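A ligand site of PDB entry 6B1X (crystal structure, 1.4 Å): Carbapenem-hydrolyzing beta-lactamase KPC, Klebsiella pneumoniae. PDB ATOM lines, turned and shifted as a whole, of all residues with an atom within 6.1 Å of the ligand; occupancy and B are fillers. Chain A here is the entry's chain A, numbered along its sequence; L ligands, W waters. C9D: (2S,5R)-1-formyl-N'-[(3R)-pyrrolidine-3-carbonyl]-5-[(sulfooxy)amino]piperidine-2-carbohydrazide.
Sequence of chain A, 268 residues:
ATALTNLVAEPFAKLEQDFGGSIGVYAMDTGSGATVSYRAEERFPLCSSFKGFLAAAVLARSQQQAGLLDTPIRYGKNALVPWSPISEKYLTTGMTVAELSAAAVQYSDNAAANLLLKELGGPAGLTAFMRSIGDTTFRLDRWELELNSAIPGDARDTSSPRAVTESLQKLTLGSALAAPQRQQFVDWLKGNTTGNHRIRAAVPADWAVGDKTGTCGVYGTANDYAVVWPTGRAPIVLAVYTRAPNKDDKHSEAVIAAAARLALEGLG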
ATOM      1  N   LEU A  46      16.237 -22.743  35.390  1.00  0.00           N
ATOM      2  CA  LEU A  46      17.363 -23.612  35.131  1.00  0.00           C
ATOM      3  C   LEU A  46      17.442 -24.098  33.697  1.00  0.00           C
ATOM      4  O   LEU A  46      18.567 -24.257  33.168  1.00  0.00           O
ATOM      5  CB  LEU A  46      17.286 -24.841  36.050  1.00  0.00           C
ATOM      6  CG  LEU A  46      17.544 -24.553  37.542  1.00  0.00           C
ATOM      7  CD1 LEU A  46      16.958 -25.652  38.411  1.00  0.00           C
ATOM      8  CD2 LEU A  46      19.038 -24.344  37.776  1.00  0.00           C
ATOM      9  N   CYS A  47      16.298 -24.361  33.079  1.00  0.00           N
ATOM     10  CA  CYS A  47      16.292 -25.044  31.764  1.00  0.00           C
ATOM     11  C   CYS A  47      17.159 -26.306  31.878  1.00  0.00           C
ATOM     12  O   CYS A  47      17.217 -26.945  32.918  1.00  0.00           O
ATOM     13  CB  CYS A  47      16.736 -24.089  30.639  1.00  0.00           C
ATOM     14  SG  CYS A  47      15.966 -22.448  30.762  1.00  0.00           S
ATOM     15  N   SER A  48      17.945 -26.618  30.836  1.00  0.00           N
ATOM     16  CA  SER A  48      18.809 -27.816  30.864  1.00  0.00           C
ATOM     17  C   SER A  48      19.901 -27.803  31.898  1.00  0.00           C
ATOM     18  O   SER A  48      20.506 -28.856  32.130  1.00  0.00           O
ATOM     19  CB  SER A  48      19.549 -28.019  29.532  1.00  0.00           C
ATOM     20  OG  SER A  48      18.696 -28.447  28.479  1.00  0.00           O
ATOM     21  N   SER A  49      20.201 -26.625  32.473  1.00  0.00           N
ATOM     22  CA  SER A  49      21.378 -26.513  33.330  1.00  0.00           C
ATOM     23  C   SER A  49      21.291 -27.377  34.588  1.00  0.00           C
ATOM     24  O   SER A  49      22.319 -27.670  35.199  1.00  0.00           O
ATOM     25  CB  SER A  49      21.732 -25.058  33.646  1.00  0.00           C
ATOM     26  OG  SER A  49      20.838 -24.496  34.580  1.00  0.00           O
ATOM     27  N   LYS A  51      21.035 -30.420  34.632  1.00  0.00           N
ATOM     28  CA  LYS A  51      21.591 -31.730  34.299  1.00  0.00           C
ATOM     29  C   LYS A  51      23.008 -31.903  34.858  1.00  0.00           C
ATOM     30  O   LYS A  51      23.420 -33.024  35.121  1.00  0.00           O
ATOM     31  CB  LYS A  51      21.559 -31.923  32.781  1.00  0.00           C
ATOM     32  CG  LYS A  51      20.151 -32.096  32.234  1.00  0.00           C
ATOM     33  CD  LYS A  51      20.078 -31.963  30.720  1.00  0.00           C
ATOM     34  CE  LYS A  51      18.633 -31.981  30.251  1.00  0.00           C
ATOM     35  NZ  LYS A  51      18.426 -31.457  28.881  1.00  0.00           N
ATOM     36  N   PRO A  82      11.963 -35.179  22.361  1.00  0.00           N
ATOM     37  CA  PRO A  82      12.928 -34.456  21.526  1.00  0.00           C
ATOM     38  C   PRO A  82      14.123 -33.891  22.281  1.00  0.00           C
ATOM     39  O   PRO A  82      14.067 -33.722  23.506  1.00  0.00           O
ATOM     40  CB  PRO A  82      12.098 -33.381  20.860  1.00  0.00           C
ATOM     41  CG  PRO A  82      10.807 -33.333  21.595  1.00  0.00           C
ATOM     42  CD  PRO A  82      10.602 -34.635  22.253  1.00  0.00           C
ATOM     43  N   TRP A  83      15.201 -33.637  21.525  1.00  0.00           N
ATOM     44  CA  TRP A  83      16.507 -33.236  22.084  1.00  0.00           C
ATOM     45  C   TRP A  83      17.070 -34.329  22.990  1.00  0.00           C
ATOM     46  O   TRP A  83      17.556 -34.049  24.106  1.00  0.00           O
ATOM     47  CB  TRP A  83      16.465 -31.854  22.761  1.00  0.00           C
ATOM     48  CG  TRP A  83      16.083 -30.708  21.864  1.00  0.00           C
ATOM     49  CD1 TRP A  83      16.932 -29.955  21.112  1.00  0.00           C
ATOM     50  CD2 TRP A  83      14.790 -30.137  21.732  1.00  0.00           C
ATOM     51  NE1 TRP A  83      16.213 -28.953  20.477  1.00  0.00           N
ATOM     52  CE2 TRP A  83      14.911 -29.029  20.856  1.00  0.00           C
ATOM     53  CE3 TRP A  83      13.528 -30.449  22.243  1.00  0.00           C
ATOM     54  CZ2 TRP A  83      13.787 -28.227  20.505  1.00  0.00           C
ATOM     55  CZ3 TRP A  83      12.442 -29.647  21.873  1.00  0.00           C
ATOM     56  CH2 TRP A  83      12.587 -28.575  21.029  1.00  0.00           C
ATOM     57  N   TYR A 107      25.644 -33.528  25.935  1.00  0.00           N
ATOM     58  CA  TYR A 107      24.728 -33.304  24.803  1.00  0.00           C
ATOM     59  C   TYR A 107      23.394 -32.786  25.287  1.00  0.00           C
ATOM     60  O   TYR A 107      22.489 -32.607  24.486  1.00  0.00           O
ATOM     61  CB  TYR A 107      24.564 -34.603  23.986  1.00  0.00           C
ATOM     62  CG  TYR A 107      25.845 -34.934  23.273  1.00  0.00           C
ATOM     63  CD1 TYR A 107      26.123 -34.364  22.036  1.00  0.00           C
ATOM     64  CD2 TYR A 107      26.800 -35.770  23.834  1.00  0.00           C
ATOM     65  CE1 TYR A 107      27.318 -34.623  21.369  1.00  0.00           C
ATOM     66  CE2 TYR A 107      28.015 -36.008  23.191  1.00  0.00           C
ATOM     67  CZ  TYR A 107      28.244 -35.445  21.968  1.00  0.00           C
ATOM     68  OH  TYR A 107      29.461 -35.676  21.312  1.00  0.00           O
ATOM     69  N   SER A 108      23.236 -32.581  26.577  1.00  0.00           N
ATOM     70  CA  SER A 108      22.015 -32.031  27.139  1.00  0.00           C
ATOM     71  C   SER A 108      20.845 -32.946  26.861  1.00  0.00           C
ATOM     72  O   SER A 108      19.708 -32.498  26.680  1.00  0.00           O
ATOM     73  CB  SER A 108      21.790 -30.608  26.662  1.00  0.00           C
ATOM     74  OG  SER A 108      21.129 -29.867  27.669  1.00  0.00           O
ATOM     75  N   ASP A 109      21.093 -34.267  26.856  1.00  0.00           N
ATOM     76  CA  ASP A 109      20.084 -35.234  26.381  1.00  0.00           C
ATOM     77  C   ASP A 109      18.894 -35.260  27.345  1.00  0.00           C
ATOM     78  O   ASP A 109      19.043 -35.555  28.535  1.00  0.00           O
ATOM     79  CB  ASP A 109      20.781 -36.597  26.278  1.00  0.00           C
ATOM     80  CG  ASP A 109      19.951 -37.680  25.629  1.00  0.00           C
ATOM     81  OD1 ASP A 109      20.398 -38.119  24.535  1.00  0.00           O
ATOM     82  OD2 ASP A 109      18.911 -38.109  26.171  1.00  0.00           O
ATOM     83  N   ASN A 110      17.713 -35.000  26.823  1.00  0.00           N
ATOM     84  CA  ASN A 110      16.525 -34.870  27.664  1.00  0.00           C
ATOM     85  C   ASN A 110      16.018 -36.194  28.263  1.00  0.00           C
ATOM     86  O   ASN A 110      15.745 -36.268  29.461  1.00  0.00           O
ATOM     87  CB  ASN A 110      15.390 -34.169  26.879  1.00  0.00           C
ATOM     88  CG  ASN A 110      15.477 -32.665  26.894  1.00  0.00           C
ATOM     89  OD1 ASN A 110      16.078 -32.040  27.776  1.00  0.00           O
ATOM     90  ND2 ASN A 110      14.795 -32.029  25.940  1.00  0.00           N
ATOM     91  N   GLU A 144      11.566 -33.194  32.216  1.00  0.00           N
ATOM     92  CA  GLU A 144      11.641 -32.789  30.811  1.00  0.00           C
ATOM     93  C   GLU A 144      10.360 -33.268  30.103  1.00  0.00           C
ATOM     94  O   GLU A 144       9.963 -34.429  30.310  1.00  0.00           O
ATOM     95  CB  GLU A 144      12.855 -33.402  30.128  1.00  0.00           C
ATOM     96  CG  GLU A 144      14.203 -32.851  30.532  1.00  0.00           C
ATOM     97  CD  GLU A 144      14.418 -31.452  30.075  1.00  0.00           C
ATOM     98  OE1 GLU A 144      13.563 -30.899  29.344  1.00  0.00           O
ATOM     99  OE2 GLU A 144      15.454 -30.866  30.428  1.00  0.00           O
ATOM    100  N   LEU A 145       9.691 -32.449  29.292  1.00  0.00           N
ATOM    101  CA  LEU A 145      10.114 -31.131  28.793  1.00  0.00           C
ATOM    102  C   LEU A 145       9.430 -29.950  29.527  1.00  0.00           C
ATOM    103  O   LEU A 145       9.737 -28.779  29.254  1.00  0.00           O
ATOM    104  CB  LEU A 145       9.714 -31.035  27.324  1.00  0.00           C
ATOM    105  CG  LEU A 145      10.098 -32.181  26.407  1.00  0.00           C
ATOM    106  CD1 LEU A 145       9.434 -32.009  25.042  1.00  0.00           C
ATOM    107  CD2 LEU A 145      11.600 -32.075  26.308  1.00  0.00           C
ATOM    108  N   GLU A 146       8.536 -30.250  30.457  1.00  0.00           N
ATOM    109  CA  GLU A 146       7.693 -29.199  31.058  1.00  0.00           C
ATOM    110  C   GLU A 146       8.502 -28.202  31.884  1.00  0.00           C
ATOM    111  O   GLU A 146       8.114 -27.043  32.038  1.00  0.00           O
ATOM    112  CB  GLU A 146       6.603 -29.820  31.925  1.00  0.00           C
ATOM    113  CG  GLU A 146       5.607 -30.700  31.164  1.00  0.00           C
ATOM    114  CD  GLU A 146       6.014 -32.164  30.950  1.00  0.00           C
ATOM    115  OE1 GLU A 146       7.134 -32.648  31.297  1.00  0.00           O
ATOM    116  OE2 GLU A 146       5.117 -32.885  30.421  1.00  0.00           O
ATOM    117  N   ASN A 148      10.923 -26.512  31.203  1.00  0.00           N
ATOM    118  CA  ASN A 148      11.438 -25.405  30.394  1.00  0.00           C
ATOM    119  C   ASN A 148      10.480 -24.274  30.154  1.00  0.00           C
ATOM    120  O   ASN A 148      10.806 -23.355  29.372  1.00  0.00           O
ATOM    121  CB  ASN A 148      11.926 -25.907  29.029  1.00  0.00           C
ATOM    122  CG  ASN A 148      13.000 -26.982  29.153  1.00  0.00           C
ATOM    123  OD1 ASN A 148      14.145 -26.668  29.478  1.00  0.00           O
ATOM    124  ND2 ASN A 148      12.635 -28.247  28.947  1.00  0.00           N
ATOM    125  N   SER A 149       9.300 -24.284  30.798  1.00  0.00           N
ATOM    126  CA  SER A 149       8.270 -23.292  30.425  1.00  0.00           C
ATOM    127  C   SER A 149       8.689 -21.853  30.684  1.00  0.00           C
ATOM    128  O   SER A 149       8.298 -20.955  29.945  1.00  0.00           O
ATOM    129  CB  SER A 149       6.933 -23.632  31.098  1.00  0.00           C
ATOM    130  OG  SER A 149       7.051 -23.808  32.486  1.00  0.00           O
ATOM    131  N   ASN A 192      31.827 -31.117  27.780  1.00  0.00           N
ATOM    132  CA  ASN A 192      30.606 -30.587  27.205  1.00  0.00           C
ATOM    133  C   ASN A 192      30.798 -30.113  25.774  1.00  0.00           C
ATOM    134  O   ASN A 192      31.826 -29.529  25.422  1.00  0.00           O
ATOM    135  CB  ASN A 192      30.072 -29.416  28.031  1.00  0.00           C
ATOM    136  CG  ASN A 192      28.770 -28.891  27.497  1.00  0.00           C
ATOM    137  OD1 ASN A 192      27.954 -29.671  27.005  1.00  0.00           O
ATOM    138  ND2 ASN A 192      28.596 -27.558  27.521  1.00  0.00           N
ATOM    139  N   THR A 194      28.136 -28.322  24.052  1.00  0.00           N
ATOM    140  CA  THR A 194      27.098 -27.323  23.740  1.00  0.00           C
ATOM    141  C   THR A 194      27.456 -25.891  24.143  1.00  0.00           C
ATOM    142  O   THR A 194      26.665 -25.004  23.925  1.00  0.00           O
ATOM    143  CB  THR A 194      25.789 -27.699  24.454  1.00  0.00           C
ATOM    144  OG1 THR A 194      25.970 -27.565  25.861  1.00  0.00           O
ATOM    145  CG2 THR A 194      25.363 -29.110  24.087  1.00  0.00           C
ATOM    146  N   ARG A 198      29.366 -19.602  24.674  1.00  0.00           N
ATOM    147  CA  ARG A 198      28.912 -18.994  25.932  1.00  0.00           C
ATOM    148  C   ARG A 198      30.126 -18.678  26.808  1.00  0.00           C
ATOM    149  O   ARG A 198      31.018 -17.971  26.325  1.00  0.00           O
ATOM    150  CB  ARG A 198      27.812 -19.883  26.542  1.00  0.00           C
ATOM    151  CG  ARG A 198      26.580 -19.831  25.682  1.00  0.00           C
ATOM    152  CD  ARG A 198      25.409 -20.570  26.319  1.00  0.00           C
ATOM    153  NE  ARG A 198      24.388 -20.747  25.290  1.00  0.00           N
ATOM    154  CZ  ARG A 198      23.157 -21.191  25.479  1.00  0.00           C
ATOM    155  NH1 ARG A 198      22.662 -21.438  26.699  1.00  0.00           N
ATOM    156  NH2 ARG A 198      22.365 -21.309  24.412  1.00  0.00           N
ATOM    157  N   LYS A 212      28.081 -26.272  31.829  1.00  0.00           N
ATOM    158  CA  LYS A 212      26.775 -26.823  31.413  1.00  0.00           C
ATOM    159  C   LYS A 212      25.873 -25.650  31.034  1.00  0.00           C
ATOM    160  O   LYS A 212      25.727 -24.691  31.801  1.00  0.00           O
ATOM    161  CB  LYS A 212      26.110 -27.625  32.553  1.00  0.00           C
ATOM    162  CG  LYS A 212      24.753 -28.232  32.164  1.00  0.00           C
ATOM    163  CD  LYS A 212      24.842 -29.408  31.218  1.00  0.00           C
ATOM    164  CE  LYS A 212      23.518 -29.688  30.513  1.00  0.00           C
ATOM    165  NZ  LYS A 212      23.266 -28.812  29.353  1.00  0.00           N
ATOM    166  N   THR A 213      25.214 -25.770  29.886  1.00  0.00           N
ATOM    167  CA  THR A 213      24.339 -24.766  29.320  1.00  0.00           C
ATOM    168  C   THR A 213      22.871 -25.099  29.555  1.00  0.00           C
ATOM    169  O   THR A 213      22.508 -26.234  29.948  1.00  0.00           O
ATOM    170  CB  THR A 213      24.579 -24.667  27.824  1.00  0.00           C
ATOM    171  OG1 THR A 213      24.389 -25.939  27.236  1.00  0.00           O
ATOM    172  CG2 THR A 213      25.958 -24.210  27.491  1.00  0.00           C
ATOM    173  N   GLY A 214      22.036 -24.098  29.340  1.00  0.00           N
ATOM    174  CA  GLY A 214      20.586 -24.268  29.344  1.00  0.00           C
ATOM    175  C   GLY A 214      19.942 -23.286  28.377  1.00  0.00           C
ATOM    176  O   GLY A 214      20.391 -22.148  28.288  1.00  0.00           O
ATOM    177  N   THR A 215      18.907 -23.706  27.666  1.00  0.00           N
ATOM    178  CA  THR A 215      18.203 -22.808  26.740  1.00  0.00           C
ATOM    179  C   THR A 215      16.729 -23.182  26.718  1.00  0.00           C
ATOM    180  O   THR A 215      16.334 -24.139  26.061  1.00  0.00           O
ATOM    181  CB  THR A 215      18.775 -22.936  25.294  1.00  0.00           C
ATOM    182  OG1 THR A 215      20.206 -22.851  25.287  1.00  0.00           O
ATOM    183  CG2 THR A 215      18.205 -21.850  24.391  1.00  0.00           C
ATOM    184  N   CYS A 216      15.899 -22.436  27.431  1.00  0.00           N
ATOM    185  CA  CYS A 216      14.448 -22.733  27.466  1.00  0.00           C
ATOM    186  C   CYS A 216      13.749 -22.419  26.122  1.00  0.00           C
ATOM    187  O   CYS A 216      12.697 -22.998  25.845  1.00  0.00           O
ATOM    188  CB  CYS A 216      13.773 -21.972  28.617  1.00  0.00           C
ATOM    189  SG  CYS A 216      13.962 -22.688  30.251  1.00  0.00           S
ATOM    190  N   GLY A 217      14.297 -21.554  25.291  1.00  0.00           N
ATOM    191  CA  GLY A 217      13.704 -21.285  23.936  1.00  0.00           C
ATOM    192  C   GLY A 217      12.497 -20.342  23.946  1.00  0.00           C
ATOM    193  O   GLY A 217      11.790 -20.200  22.929  1.00  0.00           O
ATOM    194  N   VAL A 218      12.261 -19.695  25.070  1.00  0.00           N
ATOM    195  CA  VAL A 218      11.203 -18.728  25.274  1.00  0.00           C
ATOM    196  C   VAL A 218      11.673 -17.719  26.321  1.00  0.00           C
ATOM    197  O   VAL A 218      12.591 -17.963  27.103  1.00  0.00           O
ATOM    198  CB  VAL A 218       9.888 -19.378  25.784  1.00  0.00           C
ATOM    199  CG1 VAL A 218       9.247 -20.234  24.693  1.00  0.00           C
ATOM    200  CG2 VAL A 218      10.103 -20.198  27.055  1.00  0.00           C
ATOM    201  N   ASN A 223      21.298 -19.871  29.695  1.00  0.00           N
ATOM    202  CA  ASN A 223      22.278 -19.771  30.755  1.00  0.00           C
ATOM    203  C   ASN A 223      23.487 -20.648  30.486  1.00  0.00           C
ATOM    204  O   ASN A 223      23.507 -21.441  29.550  1.00  0.00           O
ATOM    205  CB  ASN A 223      21.584 -20.128  32.087  1.00  0.00           C
ATOM    206  CG  ASN A 223      20.879 -21.465  32.011  1.00  0.00           C
ATOM    207  OD1 ASN A 223      21.515 -22.487  31.811  1.00  0.00           O
ATOM    208  ND2 ASN A 223      19.578 -21.476  32.222  1.00  0.00           N
HETATM  209  OAF C9D L   1      22.702 -27.258  25.506  1.00  0.00           O
HETATM  210  SAY C9D L   1      21.360 -26.654  25.817  1.00  0.00           S
HETATM  211  OAD C9D L   1      21.085 -27.267  27.152  1.00  0.00           O
HETATM  212  OAE C9D L   1      21.440 -25.164  25.881  1.00  0.00           O
HETATM  213  OAR C9D L   1      20.286 -27.036  24.800  1.00  0.00           O
HETATM  214  NAQ C9D L   1      20.162 -28.474  24.603  1.00  0.00           N
HETATM  215  CAU C9D L   1      18.755 -28.948  24.499  1.00  0.00           C
HETATM  216  CAJ C9D L   1      17.809 -28.082  23.675  1.00  0.00           C
HETATM  217  CB  C9D L   1      17.380 -26.884  24.425  1.00  0.00           C
HETATM  218  CAM C9D L   1      18.073 -29.235  25.883  1.00  0.00           C
HETATM  219  N   C9D L   1      17.557 -27.957  26.510  1.00  0.00           N
HETATM  220  CAG C9D L   1      18.032 -27.466  27.658  1.00  0.00           C
HETATM  221  OAA C9D L   1      17.888 -26.327  28.101  1.00  0.00           O
HETATM  222  CA  C9D L   1      16.579 -27.295  25.676  1.00  0.00           C
HETATM  223  C   C9D L   1      15.348 -27.893  25.592  1.00  0.00           C
HETATM  224  O   C9D L   1      15.037 -28.931  26.208  1.00  0.00           O
HETATM  225  NAP C9D L   1      14.531 -27.395  24.628  1.00  0.00           N
HETATM  226  NAO C9D L   1      13.246 -27.957  24.516  1.00  0.00           N
HETATM  227  CAS C9D L   1      12.228 -27.255  25.066  1.00  0.00           C
HETATM  228  OAB C9D L   1      12.350 -26.458  25.986  1.00  0.00           O
HETATM  229  CAV C9D L   1      10.840 -27.755  24.660  1.00  0.00           C
HETATM  230  CAI C9D L   1      10.304 -26.922  23.522  1.00  0.00           C
HETATM  231  CAH C9D L   1       9.692 -25.749  24.197  1.00  0.00           C
HETATM  232  NAN C9D L   1       9.307 -26.190  25.559  1.00  0.00           N
HETATM  233  CAL C9D L   1       9.823 -27.552  25.752  1.00  0.00           C
HETATM  234  O   HOH W   1       8.474 -26.336  28.385  1.00  0.00           O
HETATM  235  O   HOH W   2      15.799 -28.748  29.014  1.00  0.00           O
HETATM  236  O   HOH W   3      14.163 -24.740  23.266  1.00  0.00           O
HETATM  237  O   HOH W   4      21.470 -28.876  21.972  1.00  0.00           O
HETATM  238  O   HOH W   5       7.778 -23.100  25.942  1.00  0.00           O
HETATM  239  O   HOH W   6      10.288 -23.777  26.660  1.00  0.00           O
HETATM  240  O   HOH W   7      24.016 -24.123  24.657  1.00  0.00           O
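Water W6 lies within hydrogen-bond range of O of Cys 216 (2.7 Å), O of Asn 148 (2.8 Å) and NAN of the ligand (2.8 Å).
Water W1 lies within hydrogen-bond range of the backbone carbonyl oxygen of Leu 145, a nitrogen (NAN) of the ligand and the backbone NH of Ser 149.
Water W3 bridges a nitrogen (NAP) of the ligand (3.0 Å) and the backbone carbonyl oxygen of Cys 216 (3.4 Å).
Water W7 lies within hydrogen-bond range of O of Thr 194 (2.9 Å), OAE of the ligand (3.0 Å), OG1 of Thr 213 (3.2 Å) and NH2 of Arg 198 (3.3 Å).
OAA of the ligand is in hydrogen-bond range of N of Ser 48, at 2.8 Å.
A carbon (CAG) of the ligand is bonded to the side-chain hydroxyl of Ser 48 (1.4 Å).
The side-chain hydroxyl (OG) of Ser 108 is in hydrogen-bond range of an oxygen (OAD) of the ligand, at 2.7 Å.
N of Thr 215 is in hydrogen-bond range of OAA of the ligand.
OG1 of Thr 215 lies within hydrogen-bond range of OAE of the ligand (2.7 Å).
An oxygen (OAF) of the ligand sits at hydrogen-bond distance from the side-chain hydroxyl of Thr 213 (2.8 Å).
The side-chain amide nitrogen (ND2) of Asn 110 sits at hydrogen-bond distance from an oxygen (O) of the ligand, 3.1 Å away.
OAB of the ligand lies close to ND2 of Asn 148, 3.5 Å away.
OG1 of Thr 194 lies close to OAF of the ligand, 3.3 Å away.
The side-chain amino group of Lys 212 lies within salt-bridge range of an oxygen (OAD) of the ligand (3.5 Å).
O of Cys 216 sits close to OAB of the ligand (3.5 Å).
Cys 47 touches the ligand (CB to OAA, 3.6 Å).
NZ of Lys 51 touches CAM of the ligand, 3.7 Å away.
CZ3 of Trp 83 touches NAO of the ligand, 3.2 Å away.
Glu 144 touches the ligand (OE1 to O, 3.98 Å).
Leu 145 touches the ligand.
C of Gly 214 touches OAE of the ligand, at 3.5 Å.
Hydrophobic or aromatic side chains that line the ligand: Trp 83 and Leu 145.
Within 4 Å of the ligand: Cys 47, Ser 48, Lys 51, Trp 83, Ser 108, Asn 110, Glu 144, Leu 145, Asn 148, Thr 194, Lys 212, Thr 213, Gly 214, Thr 215 and Cys 216.
The nearest printed residue that does not touch the ligand is Arg 198 (4.01 Å).
The side-chain hydroxyl (OG) of Ser 48 lies within hydrogen-bond range of the side-chain hydroxyl (OG) of Ser 108 (2.9 Å).
The guanidinium group of Arg 198 lies within hydrogen-bond range of the side-chain hydroxyl of Thr 215 (2.8 Å).
The side-chain hydroxyl (OG1) of Thr 194 is in hydrogen-bond range of the side-chain hydroxyl (OG1) of Thr 213, 2.7 Å away.
OE2 of Glu 144 sits close to OD1 of Asn 110.
ND2 of Asn 110 lies within hydrogen-bond range of O of Pro 82, 3.1 Å away.
The backbone carbonyl oxygen (O) of Leu 145 is in hydrogen-bond range of the side-chain amide nitrogen (ND2) of Asn 148.
The guanidinium group (NH1) of Arg 198 sits at hydrogen-bond distance from the backbone carbonyl oxygen (O) of Gly 214 (2.9 Å).
The side-chain sulfur (SG) of Cys 216 is disulfide-bonded to the side-chain sulfur (SG) of Cys 47 (2.1 Å).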
